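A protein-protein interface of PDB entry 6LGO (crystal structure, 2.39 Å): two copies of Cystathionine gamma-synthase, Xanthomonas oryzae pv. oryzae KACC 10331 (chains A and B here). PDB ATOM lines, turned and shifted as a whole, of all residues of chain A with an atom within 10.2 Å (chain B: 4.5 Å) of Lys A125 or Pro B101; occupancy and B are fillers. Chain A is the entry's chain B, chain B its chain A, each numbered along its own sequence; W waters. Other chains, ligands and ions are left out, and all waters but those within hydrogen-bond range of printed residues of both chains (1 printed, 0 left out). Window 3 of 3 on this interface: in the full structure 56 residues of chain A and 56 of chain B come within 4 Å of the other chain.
The backbone carbonyl oxygen (O) of Asn B96 lies within hydrogen-bond range of the side-chain amino group (NZ) of Lys A125, at 2.4 Å.
The backbone carbonyl oxygen of Leu B99 lies within hydrogen-bond range of the side-chain amino group of Lys A125, 2.7 Å away.
O of Leu A122 lies within hydrogen-bond range of N of His A127, at 3.1 Å.
CB of Ala A121 touches CH2 of Trp B236 (3.9 Å).
O of Lys A125 touches CD of Pro B101, at 3.0 Å.
Trp B236 touches Lys A125.
His A127 touches Asn B96.
CE1 of His A127 touches CE1 of His B127 (3.4 Å).
Of the printed residues of chain B, Ala A121 touches Trp B236.
Lys A125 touches just these residues of chain B: Asn B96, Leu B99, Pro B101 and Trp B236.
Of the printed residues of chain A, Asn B96 touches Lys A125 (2.4 Å) and His A127 (3.99 Å).
No residue of chain A comes within 4 Å of Ala B97.
Of the printed residues of chain A, Leu B99 touches Lys A125 (2.7 Å).
Of chain A, only Lys A125 (3.0 Å) comes within 4 Å of Pro B101.
No residue of chain A comes within 4 Å of Gly B102.
Printed residues of chain A within 4 Å of His B127: His A127 (3.4 Å).
Printed residues of chain A within 4 Å of Trp B236: Ala A121 and Lys A125.
The nearest residue of chain B that does not touch Lys A125 is Ala B97 (4.3 Å).
Of the 10 printed residues of chain B, 5 touch a printed residue of chain A.
Printed residues of chain B that touch a printed residue of chain A: Asn B96, Leu B99, Pro B101, His B127 and Trp B236.
Of the 18 printed residues of chain A, 3 touch a printed residue of chain B.
His A127 touches its own counterpart, His B127.
Of the 7 pairs that touch across the chains among the printed residues, 1 has its exchanged pair printed and touching as well.
Water W1 lies within hydrogen-bond range of the backbone carbonyl oxygen (O) of His B127 (2.8 Å), a ring nitrogen (NE2) of His A127 (2.9 Å) and the backbone carbonyl oxygen (O) of Leu B99 (3.4 Å).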
ATOM      1  N   ASN A  92       6.078 -36.766  -5.625  1.00  0.00           N
ATOM      2  CA  ASN A  92       4.960 -36.190  -4.858  1.00  0.00           C
ATOM      3  C   ASN A  92       5.189 -36.442  -3.353  1.00  0.00           C
ATOM      4  O   ASN A  92       4.998 -35.562  -2.552  1.00  0.00           O
ATOM      5  CB  ASN A  92       3.660 -36.754  -5.361  1.00  0.00           C
ATOM      6  CG  ASN A  92       2.492 -36.076  -4.668  1.00  0.00           C
ATOM      7  OD1 ASN A  92       2.425 -34.854  -4.526  1.00  0.00           O
ATOM      8  ND2 ASN A  92       1.532 -36.855  -4.343  1.00  0.00           N
ATOM      9  N   GLN A 100       6.333 -26.946   2.738  1.00  0.00           N
ATOM     10  CA  GLN A 100       5.056 -26.271   3.105  1.00  0.00           C
ATOM     11  C   GLN A 100       5.060 -24.882   2.505  1.00  0.00           C
ATOM     12  O   GLN A 100       6.100 -24.453   2.012  1.00  0.00           O
ATOM     13  CB  GLN A 100       4.866 -26.195   4.622  1.00  0.00           C
ATOM     14  CG  GLN A 100       6.063 -25.664   5.366  1.00  0.00           C
ATOM     15  CD  GLN A 100       5.718 -25.481   6.821  1.00  0.00           C
ATOM     16  OE1 GLN A 100       6.517 -24.980   7.568  1.00  0.00           O
ATOM     17  NE2 GLN A 100       4.544 -25.906   7.249  1.00  0.00           N
ATOM     18  N   PRO A 101       3.880 -24.229   2.397  1.00  0.00           N
ATOM     19  CA  PRO A 101       3.772 -22.863   1.844  1.00  0.00           C
ATOM     20  C   PRO A 101       4.820 -21.924   2.441  1.00  0.00           C
ATOM     21  O   PRO A 101       5.102 -22.071   3.642  1.00  0.00           O
ATOM     22  CB  PRO A 101       2.353 -22.463   2.202  1.00  0.00           C
ATOM     23  CG  PRO A 101       1.628 -23.826   2.019  1.00  0.00           C
ATOM     24  CD  PRO A 101       2.568 -24.831   2.662  1.00  0.00           C
ATOM     25  N   GLY A 102       5.477 -21.130   1.596  1.00  0.00           N
ATOM     26  CA  GLY A 102       6.537 -20.243   2.083  1.00  0.00           C
ATOM     27  C   GLY A 102       7.921 -20.853   1.927  1.00  0.00           C
ATOM     28  O   GLY A 102       8.836 -20.096   1.909  1.00  0.00           O
ATOM     29  N   ARG A 117       5.807 -30.661 -14.951  1.00  0.00           N
ATOM     30  CA  ARG A 117       4.334 -30.444 -14.867  1.00  0.00           C
ATOM     31  C   ARG A 117       3.887 -30.353 -13.391  1.00  0.00           C
ATOM     32  O   ARG A 117       3.074 -29.521 -13.071  1.00  0.00           O
ATOM     33  CB  ARG A 117       3.572 -31.548 -15.583  1.00  0.00           C
ATOM     34  CG  ARG A 117       2.062 -31.475 -15.383  1.00  0.00           C
ATOM     35  CD  ARG A 117       1.458 -32.617 -16.130  1.00  0.00           C
ATOM     36  NE  ARG A 117       2.052 -33.923 -15.793  1.00  0.00           N
ATOM     37  CZ  ARG A 117       2.082 -34.974 -16.614  1.00  0.00           C
ATOM     38  NH1 ARG A 117       1.510 -34.896 -17.807  1.00  0.00           N
ATOM     39  NH2 ARG A 117       2.699 -36.085 -16.246  1.00  0.00           N
ATOM     40  N   LEU A 118       4.425 -31.202 -12.529  1.00  0.00           N
ATOM     41  CA  LEU A 118       3.997 -31.282 -11.128  1.00  0.00           C
ATOM     42  C   LEU A 118       4.569 -30.072 -10.382  1.00  0.00           C
ATOM     43  O   LEU A 118       3.798 -29.405  -9.618  1.00  0.00           O
ATOM     44  CB  LEU A 118       4.494 -32.603 -10.529  1.00  0.00           C
ATOM     45  CG  LEU A 118       4.062 -32.828  -9.078  1.00  0.00           C
ATOM     46  CD1 LEU A 118       2.568 -32.688  -8.929  1.00  0.00           C
ATOM     47  CD2 LEU A 118       4.513 -34.156  -8.538  1.00  0.00           C
ATOM     48  N   PHE A 119       5.871 -29.813 -10.529  1.00  0.00           N
ATOM     49  CA  PHE A 119       6.450 -28.618  -9.867  1.00  0.00           C
ATOM     50  C   PHE A 119       5.568 -27.384 -10.171  1.00  0.00           C
ATOM     51  O   PHE A 119       5.224 -26.665  -9.249  1.00  0.00           O
ATOM     52  CB  PHE A 119       7.905 -28.338 -10.241  1.00  0.00           C
ATOM     53  CG  PHE A 119       8.841 -29.487 -10.107  1.00  0.00           C
ATOM     54  CD1 PHE A 119       8.716 -30.402  -9.067  1.00  0.00           C
ATOM     55  CD2 PHE A 119       9.838 -29.654 -11.038  1.00  0.00           C
ATOM     56  CE1 PHE A 119       9.594 -31.473  -8.949  1.00  0.00           C
ATOM     57  CE2 PHE A 119      10.728 -30.707 -10.931  1.00  0.00           C
ATOM     58  CZ  PHE A 119      10.596 -31.627  -9.896  1.00  0.00           C
ATOM     59  N   ASN A 120       5.222 -27.166 -11.424  1.00  0.00           N
ATOM     60  CA  ASN A 120       4.607 -25.912 -11.933  1.00  0.00           C
ATOM     61  C   ASN A 120       3.158 -25.909 -11.470  1.00  0.00           C
ATOM     62  O   ASN A 120       2.768 -24.889 -10.953  1.00  0.00           O
ATOM     63  CB  ASN A 120       4.963 -25.681 -13.412  1.00  0.00           C
ATOM     64  CG  ASN A 120       6.443 -25.228 -13.559  1.00  0.00           C
ATOM     65  OD1 ASN A 120       7.453 -26.040 -13.607  1.00  0.00           O
ATOM     66  ND2 ASN A 120       6.612 -23.906 -13.537  1.00  0.00           N
ATOM     67  N   ALA A 121       2.458 -27.055 -11.428  1.00  0.00           N
ATOM     68  CA  ALA A 121       1.045 -27.078 -10.984  1.00  0.00           C
ATOM     69  C   ALA A 121       0.981 -26.808  -9.470  1.00  0.00           C
ATOM     70  O   ALA A 121       0.098 -26.020  -9.044  1.00  0.00           O
ATOM     71  CB  ALA A 121       0.373 -28.368 -11.393  1.00  0.00           C
ATOM     72  N   LEU A 122       1.890 -27.392  -8.670  1.00  0.00           N
ATOM     73  CA  LEU A 122       1.817 -27.255  -7.199  1.00  0.00           C
ATOM     74  C   LEU A 122       2.312 -25.852  -6.820  1.00  0.00           C
ATOM     75  O   LEU A 122       1.722 -25.259  -5.886  1.00  0.00           O
ATOM     76  CB  LEU A 122       2.627 -28.351  -6.503  1.00  0.00           C
ATOM     77  CG  LEU A 122       2.083 -29.791  -6.573  1.00  0.00           C
ATOM     78  CD1 LEU A 122       2.900 -30.740  -5.731  1.00  0.00           C
ATOM     79  CD2 LEU A 122       0.653 -29.897  -6.131  1.00  0.00           C
ATOM     80  N   ALA A 123       3.292 -25.277  -7.535  1.00  0.00           N
ATOM     81  CA  ALA A 123       3.713 -23.852  -7.322  1.00  0.00           C
ATOM     82  C   ALA A 123       2.576 -22.873  -7.704  1.00  0.00           C
ATOM     83  O   ALA A 123       2.360 -22.016  -6.904  1.00  0.00           O
ATOM     84  CB  ALA A 123       5.018 -23.464  -8.020  1.00  0.00           C
ATOM     85  N   LYS A 124       1.837 -23.044  -8.801  1.00  0.00           N
ATOM     86  CA  LYS A 124       0.736 -22.143  -9.140  1.00  0.00           C
ATOM     87  C   LYS A 124      -0.272 -22.130  -7.973  1.00  0.00           C
ATOM     88  O   LYS A 124      -0.771 -21.131  -7.686  1.00  0.00           O
ATOM     89  CB  LYS A 124       0.030 -22.603 -10.406  1.00  0.00           C
ATOM     90  CG  LYS A 124       0.523 -21.977 -11.715  1.00  0.00           C
ATOM     91  CD  LYS A 124      -0.445 -22.249 -12.910  1.00  0.00           C
ATOM     92  CE  LYS A 124      -1.913 -22.112 -12.510  1.00  0.00           C
ATOM     93  NZ  LYS A 124      -2.836 -22.461 -13.614  1.00  0.00           N
ATOM     94  N   LYS A 125      -0.535 -23.242  -7.323  1.00  0.00           N
ATOM     95  CA  LYS A 125      -1.418 -23.308  -6.143  1.00  0.00           C
ATOM     96  C   LYS A 125      -0.784 -22.672  -4.892  1.00  0.00           C
ATOM     97  O   LYS A 125      -1.476 -22.555  -3.904  1.00  0.00           O
ATOM     98  CB  LYS A 125      -1.736 -24.773  -5.789  1.00  0.00           C
ATOM     99  CG  LYS A 125      -2.606 -25.539  -6.758  1.00  0.00           C
ATOM    100  CD  LYS A 125      -3.387 -26.662  -6.094  1.00  0.00           C
ATOM    101  CE  LYS A 125      -4.505 -27.041  -7.045  1.00  0.00           C
ATOM    102  NZ  LYS A 125      -5.465 -27.896  -6.350  1.00  0.00           N
ATOM    103  N   GLY A 126       0.496 -22.344  -4.872  1.00  0.00           N
ATOM    104  CA  GLY A 126       1.159 -21.802  -3.675  1.00  0.00           C
ATOM    105  C   GLY A 126       1.493 -22.862  -2.635  1.00  0.00           C
ATOM    106  O   GLY A 126       1.660 -22.483  -1.485  1.00  0.00           O
ATOM    107  N   HIS A 127       1.756 -24.116  -3.002  1.00  0.00           N
ATOM    108  CA  HIS A 127       2.237 -25.125  -2.009  1.00  0.00           C
ATOM    109  C   HIS A 127       3.686 -24.809  -1.651  1.00  0.00           C
ATOM    110  O   HIS A 127       4.142 -25.252  -0.604  1.00  0.00           O
ATOM    111  CB  HIS A 127       2.071 -26.585  -2.501  1.00  0.00           C
ATOM    112  CG  HIS A 127       0.686 -27.121  -2.478  1.00  0.00           C
ATOM    113  ND1 HIS A 127       0.427 -28.463  -2.667  1.00  0.00           N
ATOM    114  CD2 HIS A 127      -0.516 -26.512  -2.330  1.00  0.00           C
ATOM    115  CE1 HIS A 127      -0.885 -28.661  -2.637  1.00  0.00           C
ATOM    116  NE2 HIS A 127      -1.497 -27.473  -2.411  1.00  0.00           N
ATOM    117  N   PHE A 128       4.413 -24.138  -2.558  1.00  0.00           N
ATOM    118  CA  PHE A 128       5.807 -23.679  -2.336  1.00  0.00           C
ATOM    119  C   PHE A 128       6.150 -22.674  -3.447  1.00  0.00           C
ATOM    120  O   PHE A 128       5.467 -22.577  -4.465  1.00  0.00           O
ATOM    121  CB  PHE A 128       6.772 -24.886  -2.308  1.00  0.00           C
ATOM    122  CG  PHE A 128       6.535 -25.887  -3.406  1.00  0.00           C
ATOM    123  CD1 PHE A 128       7.060 -25.683  -4.671  1.00  0.00           C
ATOM    124  CD2 PHE A 128       5.798 -27.044  -3.179  1.00  0.00           C
ATOM    125  CE1 PHE A 128       6.792 -26.572  -5.716  1.00  0.00           C
ATOM    126  CE2 PHE A 128       5.599 -27.978  -4.206  1.00  0.00           C
ATOM    127  CZ  PHE A 128       6.062 -27.721  -5.478  1.00  0.00           C
ATOM    128  N   ALA A 129       7.202 -21.918  -3.247  1.00  0.00           N
ATOM    129  CA  ALA A 129       7.756 -21.092  -4.313  1.00  0.00           C
ATOM    130  C   ALA A 129       8.772 -21.972  -5.060  1.00  0.00           C
ATOM    131  O   ALA A 129       9.519 -22.761  -4.392  1.00  0.00           O
ATOM    132  CB  ALA A 129       8.409 -19.858  -3.726  1.00  0.00           C
ATOM    133  N   LEU A 130       8.829 -21.778  -6.363  1.00  0.00           N
ATOM    134  CA  LEU A 130       9.606 -22.592  -7.301  1.00  0.00           C
ATOM    135  C   LEU A 130      10.747 -21.732  -7.868  1.00  0.00           C
ATOM    136  O   LEU A 130      10.422 -20.674  -8.451  1.00  0.00           O
ATOM    137  CB  LEU A 130       8.697 -22.984  -8.465  1.00  0.00           C
ATOM    138  CG  LEU A 130       8.885 -24.350  -9.102  1.00  0.00           C
ATOM    139  CD1 LEU A 130       8.653 -24.261 -10.594  1.00  0.00           C
ATOM    140  CD2 LEU A 130      10.152 -25.105  -8.748  1.00  0.00           C
ATOM    141  N   ASN B  96      -6.541 -32.330  -3.741  1.00  0.00           N
ATOM    142  CA  ASN B  96      -5.625 -31.686  -4.696  1.00  0.00           C
ATOM    143  C   ASN B  96      -6.412 -31.250  -5.928  1.00  0.00           C
ATOM    144  O   ASN B  96      -6.074 -30.262  -6.469  1.00  0.00           O
ATOM    145  CB  ASN B  96      -4.541 -32.649  -5.152  1.00  0.00           C
ATOM    146  CG  ASN B  96      -3.402 -32.706  -4.159  1.00  0.00           C
ATOM    147  OD1 ASN B  96      -2.466 -31.922  -4.318  1.00  0.00           O
ATOM    148  ND2 ASN B  96      -3.473 -33.619  -3.182  1.00  0.00           N
ATOM    149  N   ALA B  97      -7.389 -31.982  -6.445  1.00  0.00           N
ATOM    150  CA  ALA B  97      -8.007 -31.483  -7.677  1.00  0.00           C
ATOM    151  C   ALA B  97      -8.868 -30.258  -7.375  1.00  0.00           C
ATOM    152  O   ALA B  97      -9.068 -29.404  -8.249  1.00  0.00           O
ATOM    153  CB  ALA B  97      -8.843 -32.543  -8.336  1.00  0.00           C
ATOM    154  N   LEU B  99      -9.221 -28.094  -4.271  1.00  0.00           N
ATOM    155  CA  LEU B  99      -8.872 -27.059  -3.259  1.00  0.00           C
ATOM    156  C   LEU B  99      -7.510 -26.404  -3.572  1.00  0.00           C
ATOM    157  O   LEU B  99      -6.584 -27.087  -4.031  1.00  0.00           O
ATOM    158  CB  LEU B  99      -8.815 -27.715  -1.863  1.00  0.00           C
ATOM    159  CG  LEU B  99     -10.133 -28.319  -1.340  1.00  0.00           C
ATOM    160  CD1 LEU B  99      -9.900 -29.071  -0.027  1.00  0.00           C
ATOM    161  CD2 LEU B  99     -11.216 -27.260  -1.175  1.00  0.00           C
ATOM    162  N   GLN B 100      -7.353 -25.150  -3.165  1.00  0.00           N
ATOM    163  CA  GLN B 100      -6.055 -24.418  -3.062  1.00  0.00           C
ATOM    164  C   GLN B 100      -6.063 -23.560  -1.810  1.00  0.00           C
ATOM    165  O   GLN B 100      -7.102 -23.463  -1.158  1.00  0.00           O
ATOM    166  CB  GLN B 100      -5.817 -23.562  -4.300  1.00  0.00           C
ATOM    167  CG  GLN B 100      -7.040 -22.759  -4.682  1.00  0.00           C
ATOM    168  CD  GLN B 100      -6.691 -21.814  -5.793  1.00  0.00           C
ATOM    169  OE1 GLN B 100      -7.522 -21.043  -6.177  1.00  0.00           O
ATOM    170  NE2 GLN B 100      -5.473 -21.837  -6.293  1.00  0.00           N
ATOM    171  N   PRO B 101      -4.881 -23.057  -1.370  1.00  0.00           N
ATOM    172  CA  PRO B 101      -4.784 -22.220  -0.160  1.00  0.00           C
ATOM    173  C   PRO B 101      -5.823 -21.092  -0.208  1.00  0.00           C
ATOM    174  O   PRO B 101      -6.066 -20.599  -1.331  1.00  0.00           O
ATOM    175  CB  PRO B 101      -3.333 -21.768  -0.211  1.00  0.00           C
ATOM    176  CG  PRO B 101      -2.641 -23.025  -0.777  1.00  0.00           C
ATOM    177  CD  PRO B 101      -3.559 -23.397  -1.923  1.00  0.00           C
ATOM    178  N   GLY B 102      -6.494 -20.827   0.923  1.00  0.00           N
ATOM    179  CA  GLY B 102      -7.598 -19.856   0.972  1.00  0.00           C
ATOM    180  C   GLY B 102      -8.974 -20.486   0.809  1.00  0.00           C
ATOM    181  O   GLY B 102      -9.916 -19.887   1.271  1.00  0.00           O
ATOM    182  N   ASP B 103      -9.123 -21.612   0.092  1.00  0.00           N
ATOM    183  CA  ASP B 103     -10.419 -22.321   0.005  1.00  0.00           C
ATOM    184  C   ASP B 103     -10.691 -22.958   1.366  1.00  0.00           C
ATOM    185  O   ASP B 103      -9.758 -23.332   2.100  1.00  0.00           O
ATOM    186  CB  ASP B 103     -10.477 -23.407  -1.073  1.00  0.00           C
ATOM    187  CG  ASP B 103     -10.322 -22.996  -2.510  1.00  0.00           C
ATOM    188  OD1 ASP B 103     -10.504 -21.812  -2.763  1.00  0.00           O
ATOM    189  OD2 ASP B 103      -9.997 -23.902  -3.367  1.00  0.00           O
ATOM    190  N   GLY B 126      -1.398 -25.497   5.770  1.00  0.00           N
ATOM    191  CA  GLY B 126      -2.051 -24.366   5.075  1.00  0.00           C
ATOM    192  C   GLY B 126      -2.450 -24.682   3.636  1.00  0.00           C
ATOM    193  O   GLY B 126      -2.687 -23.759   2.867  1.00  0.00           O
ATOM    194  N   HIS B 127      -2.704 -25.929   3.283  1.00  0.00           N
ATOM    195  CA  HIS B 127      -3.200 -26.239   1.914  1.00  0.00           C
ATOM    196  C   HIS B 127      -4.640 -25.769   1.771  1.00  0.00           C
ATOM    197  O   HIS B 127      -5.088 -25.627   0.673  1.00  0.00           O
ATOM    198  CB  HIS B 127      -3.044 -27.732   1.557  1.00  0.00           C
ATOM    199  CG  HIS B 127      -1.652 -28.164   1.261  1.00  0.00           C
ATOM    200  ND1 HIS B 127      -1.379 -29.390   0.682  1.00  0.00           N
ATOM    201  CD2 HIS B 127      -0.458 -27.568   1.465  1.00  0.00           C
ATOM    202  CE1 HIS B 127      -0.067 -29.523   0.541  1.00  0.00           C
ATOM    203  NE2 HIS B 127       0.515 -28.414   0.987  1.00  0.00           N
ATOM    204  N   TRP B 236      -5.073 -34.776 -12.609  1.00  0.00           N
ATOM    205  CA  TRP B 236      -4.377 -34.645 -11.324  1.00  0.00           C
ATOM    206  C   TRP B 236      -3.858 -36.014 -10.919  1.00  0.00           C
ATOM    207  O   TRP B 236      -2.770 -36.094 -10.373  1.00  0.00           O
ATOM    208  CB  TRP B 236      -5.341 -34.031 -10.278  1.00  0.00           C
ATOM    209  CG  TRP B 236      -5.320 -32.531 -10.342  1.00  0.00           C
ATOM    210  CD1 TRP B 236      -6.282 -31.717 -10.888  1.00  0.00           C
ATOM    211  CD2 TRP B 236      -4.272 -31.650  -9.901  1.00  0.00           C
ATOM    212  NE1 TRP B 236      -5.900 -30.412 -10.822  1.00  0.00           N
ATOM    213  CE2 TRP B 236      -4.676 -30.331 -10.224  1.00  0.00           C
ATOM    214  CE3 TRP B 236      -3.035 -31.846  -9.282  1.00  0.00           C
ATOM    215  CZ2 TRP B 236      -3.894 -29.203  -9.956  1.00  0.00           C
ATOM    216  CZ3 TRP B 236      -2.261 -30.734  -9.006  1.00  0.00           C
ATOM    217  CH2 TRP B 236      -2.703 -29.435  -9.311  1.00  0.00           C
HETATM  218  O   HOH W   1      -4.188 -26.816  -1.652  1.00  0.00           O
